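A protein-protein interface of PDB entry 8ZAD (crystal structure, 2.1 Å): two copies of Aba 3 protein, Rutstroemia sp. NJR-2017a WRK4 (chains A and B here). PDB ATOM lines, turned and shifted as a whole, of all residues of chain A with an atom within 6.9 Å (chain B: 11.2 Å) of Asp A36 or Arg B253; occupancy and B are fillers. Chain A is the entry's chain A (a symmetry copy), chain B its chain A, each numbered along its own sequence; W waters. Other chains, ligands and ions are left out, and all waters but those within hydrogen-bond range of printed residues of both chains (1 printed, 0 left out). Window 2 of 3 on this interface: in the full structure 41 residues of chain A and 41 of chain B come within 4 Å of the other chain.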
ATOM      1  N   TYR A  33      20.748 -16.443   4.208  1.00  0.00           N
ATOM      2  CA  TYR A  33      22.132 -16.847   4.558  1.00  0.00           C
ATOM      3  C   TYR A  33      22.655 -17.666   3.392  1.00  0.00           C
ATOM      4  O   TYR A  33      21.872 -18.196   2.631  1.00  0.00           O
ATOM      5  CB  TYR A  33      22.155 -17.666   5.849  1.00  0.00           C
ATOM      6  CG  TYR A  33      21.127 -18.771   5.914  1.00  0.00           C
ATOM      7  CD1 TYR A  33      21.403 -20.042   5.433  1.00  0.00           C
ATOM      8  CD2 TYR A  33      19.880 -18.543   6.472  1.00  0.00           C
ATOM      9  CE1 TYR A  33      20.472 -21.059   5.507  1.00  0.00           C
ATOM     10  CE2 TYR A  33      18.927 -19.538   6.534  1.00  0.00           C
ATOM     11  CZ  TYR A  33      19.226 -20.799   6.054  1.00  0.00           C
ATOM     12  OH  TYR A  33      18.286 -21.778   6.152  1.00  0.00           O
ATOM     13  N   PRO A  34      23.981 -17.804   3.228  1.00  0.00           N
ATOM     14  CA  PRO A  34      24.519 -18.571   2.115  1.00  0.00           C
ATOM     15  C   PRO A  34      24.238 -20.056   2.296  1.00  0.00           C
ATOM     16  O   PRO A  34      24.056 -20.544   3.415  1.00  0.00           O
ATOM     17  CB  PRO A  34      26.002 -18.208   2.148  1.00  0.00           C
ATOM     18  CG  PRO A  34      26.268 -17.862   3.587  1.00  0.00           C
ATOM     19  CD  PRO A  34      25.008 -17.196   4.077  1.00  0.00           C
ATOM     20  N   PRO A  35      24.071 -20.816   1.192  1.00  0.00           N
ATOM     21  CA  PRO A  35      23.713 -22.229   1.302  1.00  0.00           C
ATOM     22  C   PRO A  35      24.838 -23.083   1.893  1.00  0.00           C
ATOM     23  O   PRO A  35      24.547 -24.137   2.359  1.00  0.00           O
ATOM     24  CB  PRO A  35      23.337 -22.577  -0.151  1.00  0.00           C
ATOM     25  CG  PRO A  35      24.160 -21.644  -0.970  1.00  0.00           C
ATOM     26  CD  PRO A  35      24.071 -20.346  -0.198  1.00  0.00           C
ATOM     27  N   ASP A  36      26.073 -22.581   1.952  1.00  0.00           N
ATOM     28  CA  ASP A  36      27.221 -23.360   2.484  1.00  0.00           C
ATOM     29  C   ASP A  36      26.949 -23.832   3.915  1.00  0.00           C
ATOM     30  O   ASP A  36      27.544 -24.875   4.316  1.00  0.00           O
ATOM     31  CB  ASP A  36      28.526 -22.564   2.474  1.00  0.00           C
ATOM     32  CG  ASP A  36      28.904 -22.025   1.109  1.00  0.00           C
ATOM     33  OD1 ASP A  36      28.081 -21.258   0.558  1.00  0.00           O
ATOM     34  OD2 ASP A  36      30.048 -22.290   0.666  1.00  0.00           O
ATOM     35  N   ILE A  37      26.201 -23.038   4.692  1.00  0.00           N
ATOM     36  CA  ILE A  37      25.918 -23.330   6.122  1.00  0.00           C
ATOM     37  C   ILE A  37      24.511 -23.912   6.293  1.00  0.00           C
ATOM     38  O   ILE A  37      24.195 -24.260   7.408  1.00  0.00           O
ATOM     39  CB  ILE A  37      26.130 -22.095   6.999  1.00  0.00           C
ATOM     40  CG1 ILE A  37      25.110 -20.978   6.716  1.00  0.00           C
ATOM     41  CG2 ILE A  37      27.574 -21.618   6.910  1.00  0.00           C
ATOM     42  CD1 ILE A  37      25.234 -19.787   7.650  1.00  0.00           C
ATOM     43  N   ALA A  38      23.734 -24.086   5.225  1.00  0.00           N
ATOM     44  CA  ALA A  38      22.305 -24.455   5.320  1.00  0.00           C
ATOM     45  C   ALA A  38      22.162 -25.856   5.922  1.00  0.00           C
ATOM     46  O   ALA A  38      21.127 -26.117   6.489  1.00  0.00           O
ATOM     47  CB  ALA A  38      21.621 -24.338   3.960  1.00  0.00           C
ATOM     48  N   SER A  39      23.147 -26.748   5.764  1.00  0.00           N
ATOM     49  CA  SER A  39      23.088 -28.120   6.319  1.00  0.00           C
ATOM     50  C   SER A  39      24.070 -28.248   7.492  1.00  0.00           C
ATOM     51  O   SER A  39      24.527 -29.367   7.776  1.00  0.00           O
ATOM     52  CB  SER A  39      23.307 -29.134   5.205  1.00  0.00           C
ATOM     53  OG  SER A  39      22.238 -29.075   4.257  1.00  0.00           O
ATOM     54  N   ASP A  40      24.385 -27.150   8.188  1.00  0.00           N
ATOM     55  CA  ASP A  40      25.223 -27.227   9.418  1.00  0.00           C
ATOM     56  C   ASP A  40      24.316 -27.666  10.579  1.00  0.00           C
ATOM     57  O   ASP A  40      23.104 -27.741  10.370  1.00  0.00           O
ATOM     58  CB  ASP A  40      25.930 -25.914   9.754  1.00  0.00           C
ATOM     59  CG  ASP A  40      27.053 -25.478   8.822  1.00  0.00           C
ATOM     60  OD1 ASP A  40      27.230 -26.090   7.768  1.00  0.00           O
ATOM     61  OD2 ASP A  40      27.712 -24.495   9.163  1.00  0.00           O
ATOM     62  N   TRP A  59      25.235 -14.835   9.366  1.00  0.00           N
ATOM     63  CA  TRP A  59      25.488 -14.183   8.065  1.00  0.00           C
ATOM     64  C   TRP A  59      25.378 -12.655   8.206  1.00  0.00           C
ATOM     65  O   TRP A  59      26.275 -11.959   7.739  1.00  0.00           O
ATOM     66  CB  TRP A  59      24.512 -14.728   7.030  1.00  0.00           C
ATOM     67  CG  TRP A  59      24.460 -13.934   5.759  1.00  0.00           C
ATOM     68  CD1 TRP A  59      23.398 -13.214   5.315  1.00  0.00           C
ATOM     69  CD2 TRP A  59      25.448 -13.882   4.717  1.00  0.00           C
ATOM     70  NE1 TRP A  59      23.673 -12.676   4.086  1.00  0.00           N
ATOM     71  CE2 TRP A  59      24.909 -13.092   3.680  1.00  0.00           C
ATOM     72  CE3 TRP A  59      26.728 -14.419   4.546  1.00  0.00           C
ATOM     73  CZ2 TRP A  59      25.627 -12.787   2.523  1.00  0.00           C
ATOM     74  CZ3 TRP A  59      27.421 -14.154   3.381  1.00  0.00           C
ATOM     75  CH2 TRP A  59      26.888 -13.322   2.388  1.00  0.00           C
ATOM     76  N   TYR A  69      35.575  -9.075   2.012  1.00  0.00           N
ATOM     77  CA  TYR A  69      36.355 -10.334   2.114  1.00  0.00           C
ATOM     78  C   TYR A  69      36.959 -10.700   0.769  1.00  0.00           C
ATOM     79  O   TYR A  69      36.402 -10.320  -0.256  1.00  0.00           O
ATOM     80  CB  TYR A  69      35.450 -11.469   2.594  1.00  0.00           C
ATOM     81  CG  TYR A  69      34.458 -11.956   1.575  1.00  0.00           C
ATOM     82  CD1 TYR A  69      33.215 -11.355   1.442  1.00  0.00           C
ATOM     83  CD2 TYR A  69      34.762 -13.030   0.752  1.00  0.00           C
ATOM     84  CE1 TYR A  69      32.293 -11.815   0.513  1.00  0.00           C
ATOM     85  CE2 TYR A  69      33.871 -13.479  -0.205  1.00  0.00           C
ATOM     86  CZ  TYR A  69      32.623 -12.884  -0.303  1.00  0.00           C
ATOM     87  OH  TYR A  69      31.723 -13.357  -1.217  1.00  0.00           O
ATOM     88  N   TRP A  72      36.513 -16.650   0.810  1.00  0.00           N
ATOM     89  CA  TRP A  72      35.179 -17.214   1.131  1.00  0.00           C
ATOM     90  C   TRP A  72      35.301 -18.310   2.199  1.00  0.00           C
ATOM     91  O   TRP A  72      34.508 -18.341   3.125  1.00  0.00           O
ATOM     92  CB  TRP A  72      34.482 -17.706  -0.145  1.00  0.00           C
ATOM     93  CG  TRP A  72      33.139 -18.285   0.149  1.00  0.00           C
ATOM     94  CD1 TRP A  72      32.806 -19.608   0.111  1.00  0.00           C
ATOM     95  CD2 TRP A  72      31.956 -17.579   0.551  1.00  0.00           C
ATOM     96  NE1 TRP A  72      31.488 -19.765   0.448  1.00  0.00           N
ATOM     97  CE2 TRP A  72      30.939 -18.544   0.706  1.00  0.00           C
ATOM     98  CE3 TRP A  72      31.637 -16.227   0.779  1.00  0.00           C
ATOM     99  CZ2 TRP A  72      29.652 -18.208   1.102  1.00  0.00           C
ATOM    100  CZ3 TRP A  72      30.345 -15.889   1.117  1.00  0.00           C
ATOM    101  CH2 TRP A  72      29.372 -16.869   1.323  1.00  0.00           C
ATOM    102  N   VAL A  76      33.316 -18.132   5.718  1.00  0.00           N
ATOM    103  CA  VAL A  76      32.380 -19.192   6.200  1.00  0.00           C
ATOM    104  C   VAL A  76      32.894 -19.728   7.536  1.00  0.00           C
ATOM    105  O   VAL A  76      32.042 -19.991   8.409  1.00  0.00           O
ATOM    106  CB  VAL A  76      32.195 -20.319   5.162  1.00  0.00           C
ATOM    107  CG1 VAL A  76      31.355 -21.465   5.717  1.00  0.00           C
ATOM    108  CG2 VAL A  76      31.575 -19.748   3.901  1.00  0.00           C
ATOM    109  N   MET A  79      31.754 -17.301  10.044  1.00  0.00           N
ATOM    110  CA  MET A  79      30.292 -17.442  10.193  1.00  0.00           C
ATOM    111  C   MET A  79      30.007 -18.588  11.169  1.00  0.00           C
ATOM    112  O   MET A  79      29.133 -18.441  12.032  1.00  0.00           O
ATOM    113  CB  MET A  79      29.594 -17.745   8.872  1.00  0.00           C
ATOM    114  CG  MET A  79      29.536 -16.572   7.941  1.00  0.00           C
ATOM    115  SD  MET A  79      28.766 -17.107   6.405  1.00  0.00           S
ATOM    116  CE  MET A  79      29.784 -16.275   5.186  1.00  0.00           C
ATOM    117  N   ARG A  80      30.770 -19.654  11.090  1.00  0.00           N
ATOM    118  CA  ARG A  80      30.549 -20.839  11.961  1.00  0.00           C
ATOM    119  C   ARG A  80      30.958 -20.526  13.398  1.00  0.00           C
ATOM    120  O   ARG A  80      30.234 -20.952  14.316  1.00  0.00           O
ATOM    121  CB  ARG A  80      31.253 -22.032  11.328  1.00  0.00           C
ATOM    122  CG  ARG A  80      30.492 -22.516  10.108  1.00  0.00           C
ATOM    123  CD  ARG A  80      31.235 -23.580   9.343  1.00  0.00           C
ATOM    124  NE  ARG A  80      30.372 -24.141   8.344  1.00  0.00           N
ATOM    125  CZ  ARG A  80      30.771 -24.738   7.245  1.00  0.00           C
ATOM    126  NH1 ARG A  80      32.048 -24.829   6.957  1.00  0.00           N
ATOM    127  NH2 ARG A  80      29.887 -25.203   6.399  1.00  0.00           N
ATOM    128  N   TRP B 245      18.850  -7.689   2.457  1.00  0.00           N
ATOM    129  CA  TRP B 245      19.469  -8.939   2.998  1.00  0.00           C
ATOM    130  C   TRP B 245      19.291 -10.105   2.004  1.00  0.00           C
ATOM    131  O   TRP B 245      20.256 -10.855   1.744  1.00  0.00           O
ATOM    132  CB  TRP B 245      18.866  -9.262   4.363  1.00  0.00           C
ATOM    133  CG  TRP B 245      19.490  -8.476   5.463  1.00  0.00           C
ATOM    134  CD1 TRP B 245      18.880  -7.668   6.375  1.00  0.00           C
ATOM    135  CD2 TRP B 245      20.882  -8.500   5.804  1.00  0.00           C
ATOM    136  NE1 TRP B 245      19.804  -7.153   7.240  1.00  0.00           N
ATOM    137  CE2 TRP B 245      21.046  -7.628   6.901  1.00  0.00           C
ATOM    138  CE3 TRP B 245      21.997  -9.163   5.278  1.00  0.00           C
ATOM    139  CZ2 TRP B 245      22.279  -7.431   7.497  1.00  0.00           C
ATOM    140  CZ3 TRP B 245      23.225  -8.922   5.841  1.00  0.00           C
ATOM    141  CH2 TRP B 245      23.362  -8.051   6.918  1.00  0.00           C
ATOM    142  N   ALA B 246      18.120 -10.223   1.386  1.00  0.00           N
ATOM    143  CA  ALA B 246      17.822 -11.313   0.424  1.00  0.00           C
ATOM    144  C   ALA B 246      18.753 -11.193  -0.789  1.00  0.00           C
ATOM    145  O   ALA B 246      19.333 -12.222  -1.237  1.00  0.00           O
ATOM    146  CB  ALA B 246      16.353 -11.285   0.045  1.00  0.00           C
ATOM    147  N   LEU B 247      18.936  -9.989  -1.306  1.00  0.00           N
ATOM    148  CA  LEU B 247      19.877  -9.728  -2.434  1.00  0.00           C
ATOM    149  C   LEU B 247      21.301 -10.115  -2.016  1.00  0.00           C
ATOM    150  O   LEU B 247      22.042 -10.750  -2.812  1.00  0.00           O
ATOM    151  CB  LEU B 247      19.823  -8.233  -2.761  1.00  0.00           C
ATOM    152  CG  LEU B 247      19.266  -7.766  -4.104  1.00  0.00           C
ATOM    153  CD1 LEU B 247      18.400  -8.780  -4.828  1.00  0.00           C
ATOM    154  CD2 LEU B 247      18.514  -6.455  -3.905  1.00  0.00           C
ATOM    155  N   ASP B 248      21.721  -9.628  -0.857  1.00  0.00           N
ATOM    156  CA  ASP B 248      23.050  -9.925  -0.255  1.00  0.00           C
ATOM    157  C   ASP B 248      23.248 -11.449  -0.272  1.00  0.00           C
ATOM    158  O   ASP B 248      24.260 -11.914  -0.763  1.00  0.00           O
ATOM    159  CB  ASP B 248      23.137  -9.329   1.147  1.00  0.00           C
ATOM    160  CG  ASP B 248      24.542  -9.051   1.659  1.00  0.00           C
ATOM    161  OD1 ASP B 248      25.493  -9.211   0.881  1.00  0.00           O
ATOM    162  OD2 ASP B 248      24.673  -8.679   2.840  1.00  0.00           O
ATOM    163  N   ALA B 249      22.275 -12.209   0.228  1.00  0.00           N
ATOM    164  CA  ALA B 249      22.380 -13.684   0.321  1.00  0.00           C
ATOM    165  C   ALA B 249      22.408 -14.297  -1.094  1.00  0.00           C
ATOM    166  O   ALA B 249      23.239 -15.157  -1.377  1.00  0.00           O
ATOM    167  CB  ALA B 249      21.254 -14.225   1.164  1.00  0.00           C
ATOM    168  N   ALA B 250      21.583 -13.794  -1.996  1.00  0.00           N
ATOM    169  CA  ALA B 250      21.535 -14.229  -3.409  1.00  0.00           C
ATOM    170  C   ALA B 250      22.822 -13.872  -4.153  1.00  0.00           C
ATOM    171  O   ALA B 250      23.090 -14.526  -5.155  1.00  0.00           O
ATOM    172  CB  ALA B 250      20.329 -13.645  -4.063  1.00  0.00           C
ATOM    173  N   TRP B 251      23.599 -12.887  -3.695  1.00  0.00           N
ATOM    174  CA  TRP B 251      24.864 -12.494  -4.355  1.00  0.00           C
ATOM    175  C   TRP B 251      26.060 -13.061  -3.600  1.00  0.00           C
ATOM    176  O   TRP B 251      27.194 -12.668  -3.920  1.00  0.00           O
ATOM    177  CB  TRP B 251      24.922 -10.973  -4.471  1.00  0.00           C
ATOM    178  CG  TRP B 251      23.863 -10.415  -5.369  1.00  0.00           C
ATOM    179  CD1 TRP B 251      22.979 -11.099  -6.159  1.00  0.00           C
ATOM    180  CD2 TRP B 251      23.571  -9.022  -5.554  1.00  0.00           C
ATOM    181  NE1 TRP B 251      22.141 -10.229  -6.811  1.00  0.00           N
ATOM    182  CE2 TRP B 251      22.503  -8.945  -6.475  1.00  0.00           C
ATOM    183  CE3 TRP B 251      24.112  -7.850  -5.024  1.00  0.00           C
ATOM    184  CZ2 TRP B 251      21.975  -7.726  -6.885  1.00  0.00           C
ATOM    185  CZ3 TRP B 251      23.591  -6.643  -5.433  1.00  0.00           C
ATOM    186  CH2 TRP B 251      22.525  -6.591  -6.330  1.00  0.00           C
ATOM    187  N   ALA B 252      25.823 -13.948  -2.631  1.00  0.00           N
ATOM    188  CA  ALA B 252      26.896 -14.543  -1.804  1.00  0.00           C
ATOM    189  C   ALA B 252      27.948 -15.189  -2.720  1.00  0.00           C
ATOM    190  O   ALA B 252      27.604 -15.754  -3.804  1.00  0.00           O
ATOM    191  CB  ALA B 252      26.347 -15.524  -0.800  1.00  0.00           C
ATOM    192  N   ARG B 253      29.187 -14.953  -2.328  1.00  0.00           N
ATOM    193  CA  ARG B 253      30.474 -15.547  -2.796  1.00  0.00           C
ATOM    194  C   ARG B 253      30.880 -14.980  -4.170  1.00  0.00           C
ATOM    195  O   ARG B 253      31.867 -15.473  -4.728  1.00  0.00           O
ATOM    196  CB  ARG B 253      30.490 -17.061  -2.525  1.00  0.00           C
ATOM    197  CG  ARG B 253      30.213 -18.036  -3.657  1.00  0.00           C
ATOM    198  CD  ARG B 253      30.780 -19.366  -3.154  1.00  0.00           C
ATOM    199  NE  ARG B 253      29.945 -20.549  -3.366  1.00  0.00           N
ATOM    200  CZ  ARG B 253      28.755 -20.783  -2.801  1.00  0.00           C
ATOM    201  NH1 ARG B 253      28.186 -19.898  -1.997  1.00  0.00           N
ATOM    202  NH2 ARG B 253      28.116 -21.905  -3.076  1.00  0.00           N
ATOM    203  N   ASN B 254      30.160 -13.947  -4.626  1.00  0.00           N
ATOM    204  CA  ASN B 254      30.618 -12.934  -5.612  1.00  0.00           C
ATOM    205  C   ASN B 254      31.018 -11.696  -4.820  1.00  0.00           C
ATOM    206  O   ASN B 254      30.205 -10.785  -4.694  1.00  0.00           O
ATOM    207  CB  ASN B 254      29.523 -12.568  -6.616  1.00  0.00           C
ATOM    208  CG  ASN B 254      28.475 -13.643  -6.807  1.00  0.00           C
ATOM    209  OD1 ASN B 254      27.530 -13.458  -7.572  1.00  0.00           O
ATOM    210  ND2 ASN B 254      28.626 -14.768  -6.127  1.00  0.00           N
ATOM    211  N   PRO B 255      32.240 -11.623  -4.235  1.00  0.00           N
ATOM    212  CA  PRO B 255      32.586 -10.505  -3.358  1.00  0.00           C
ATOM    213  C   PRO B 255      32.649  -9.157  -4.084  1.00  0.00           C
ATOM    214  O   PRO B 255      32.869  -8.169  -3.422  1.00  0.00           O
ATOM    215  CB  PRO B 255      33.977 -10.864  -2.790  1.00  0.00           C
ATOM    216  CG  PRO B 255      34.547 -11.890  -3.766  1.00  0.00           C
ATOM    217  CD  PRO B 255      33.350 -12.584  -4.386  1.00  0.00           C
ATOM    218  N   LYS B 256      32.489  -9.156  -5.405  1.00  0.00           N
ATOM    219  CA  LYS B 256      32.447  -7.918  -6.232  1.00  0.00           C
ATOM    220  C   LYS B 256      31.231  -7.123  -5.780  1.00  0.00           C
ATOM    221  O   LYS B 256      31.392  -5.915  -5.372  1.00  0.00           O
ATOM    222  CB  LYS B 256      32.390  -8.259  -7.726  1.00  0.00           C
ATOM    223  CG  LYS B 256      33.724  -8.754  -8.274  1.00  0.00           C
ATOM    224  CD  LYS B 256      33.721  -9.127  -9.740  1.00  0.00           C
ATOM    225  CE  LYS B 256      35.125  -9.448 -10.207  1.00  0.00           C
ATOM    226  NZ  LYS B 256      35.161  -9.706 -11.663  1.00  0.00           N
ATOM    227  N   LEU B 257      30.116  -7.844  -5.680  1.00  0.00           N
ATOM    228  CA  LEU B 257      28.785  -7.243  -5.522  1.00  0.00           C
ATOM    229  C   LEU B 257      28.601  -6.734  -4.099  1.00  0.00           C
ATOM    230  O   LEU B 257      27.696  -5.871  -3.933  1.00  0.00           O
ATOM    231  CB  LEU B 257      27.719  -8.248  -5.936  1.00  0.00           C
ATOM    232  CG  LEU B 257      27.743  -8.635  -7.408  1.00  0.00           C
ATOM    233  CD1 LEU B 257      26.473  -9.398  -7.768  1.00  0.00           C
ATOM    234  CD2 LEU B 257      27.921  -7.439  -8.326  1.00  0.00           C
ATOM    235  N   VAL B 258      29.459  -7.129  -3.146  1.00  0.00           N
ATOM    236  CA  VAL B 258      29.340  -6.603  -1.752  1.00  0.00           C
ATOM    237  C   VAL B 258      29.541  -5.084  -1.754  1.00  0.00           C
ATOM    238  O   VAL B 258      28.998  -4.450  -0.847  1.00  0.00           O
ATOM    239  CB  VAL B 258      30.259  -7.295  -0.723  1.00  0.00           C
ATOM    240  CG1 VAL B 258      30.042  -8.788  -0.745  1.00  0.00           C
ATOM    241  CG2 VAL B 258      31.724  -6.942  -0.900  1.00  0.00           C
ATOM    242  N   ASN B 259      30.307  -4.506  -2.691  1.00  0.00           N
ATOM    243  CA  ASN B 259      30.492  -3.025  -2.770  1.00  0.00           C
ATOM    244  C   ASN B 259      29.159  -2.324  -3.045  1.00  0.00           C
ATOM    245  O   ASN B 259      28.953  -1.199  -2.497  1.00  0.00           O
ATOM    246  CB  ASN B 259      31.557  -2.623  -3.770  1.00  0.00           C
ATOM    247  CG  ASN B 259      32.868  -3.267  -3.386  1.00  0.00           C
ATOM    248  OD1 ASN B 259      33.351  -3.025  -2.287  1.00  0.00           O
ATOM    249  ND2 ASN B 259      33.320  -4.217  -4.189  1.00  0.00           N
ATOM    250  N   ILE B 261      25.950  -3.773  -2.282  1.00  0.00           N
ATOM    251  CA  ILE B 261      25.170  -4.010  -1.037  1.00  0.00           C
ATOM    252  C   ILE B 261      25.669  -3.044   0.054  1.00  0.00           C
ATOM    253  O   ILE B 261      24.834  -2.387   0.692  1.00  0.00           O
ATOM    254  CB  ILE B 261      25.283  -5.463  -0.579  1.00  0.00           C
ATOM    255  CG1 ILE B 261      24.769  -6.451  -1.639  1.00  0.00           C
ATOM    256  CG2 ILE B 261      24.619  -5.621   0.793  1.00  0.00           C
ATOM    257  CD1 ILE B 261      23.277  -6.638  -1.657  1.00  0.00           C
HETATM  258  O   HOH W   1      31.572 -22.035  -1.931  1.00  0.00           O
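Among the printed residues, merely in contact across the chains: Trp A72 with Arg B253, Tyr A69 with Pro B255, Trp A59 with Asp B248, Tyr A69 with Asn B254, Tyr A33 with Ala B249, Trp A59 with Ala B252, Trp A72 with Ala B252 and Tyr A69 with Val B258.
The guanidinium group of Arg B253 is in salt-bridge range of the side-chain carboxylate of Asp A36.
N of Arg B253 lies close to OH of Tyr A69 (3.2 Å).
No residue of chain B comes within 4 Å of Pro A35.
Asp A36 touches just one residue of chain B: Arg B253.
No residue of chain B comes within 4 Å of Ala A38.
Ser A39 touches none of the printed residues of chain B.
Printed residues of chain B within 4 Å of Tyr A69: Arg B253, Asn B254, Pro B255 and Val B258.
Trp A72 touches just these residues of chain B: Ala B252 and Arg B253.
Val A76 touches none of the printed residues of chain B.
Of the printed residues of chain A, Asp B248 touches Trp A59 (3.7 Å).
Of the printed residues of chain A, Ala B252 touches Trp A59 (3.9 Å) and Trp A72 (3.9 Å).
Of chain A, only Asp A36, Tyr A69 and Trp A72 come within 4 Å of Arg B253.
Printed residues of chain A within 4 Å of Pro B255: Tyr A69 (3.5 Å).
The nearest residue of chain B that does not touch Asp A36 is Ala B252 (6.1 Å).
The nearest residue of chain A that does not touch Arg B253 is Pro A35 (4.5 Å).
Water W1 lies within hydrogen-bond range of NE of Arg B253 (2.6 Å), OD2 of Asp A36 (3.0 Å) and NE1 of Trp A72 (3.3 Å).
O of Trp B251 lies close to ND2 of Asn B254 (3.4 Å).
The side-chain amide nitrogen of Asn B254 is in hydrogen-bond range of the backbone carbonyl oxygen of Ala B252 (2.7 Å).
The side-chain carboxylate (OD2) of Asp A36 lies within hydrogen-bond range of the indole nitrogen (NE1) of Trp A72 (2.9 Å).
The backbone carbonyl oxygen of Asp A36 is in hydrogen-bond range of the guanidinium group of Arg A80.
No position is printed for both chains.
Of the 10 pairs that touch across the chains among the printed residues, none has its exchanged pair printed and touching as well.
Of the 16 printed residues of chain B, 7 touch a printed residue of chain A.
Hydrophobic or aromatic side chains of chain B within 4 Å of the printed part of chain A: Ala B249, Ala B252, Pro B255 and Val B258.
Of the 14 printed residues of chain A, 5 touch a printed residue of chain B.
Among the printed residues, 10 pairs touch across the chains.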
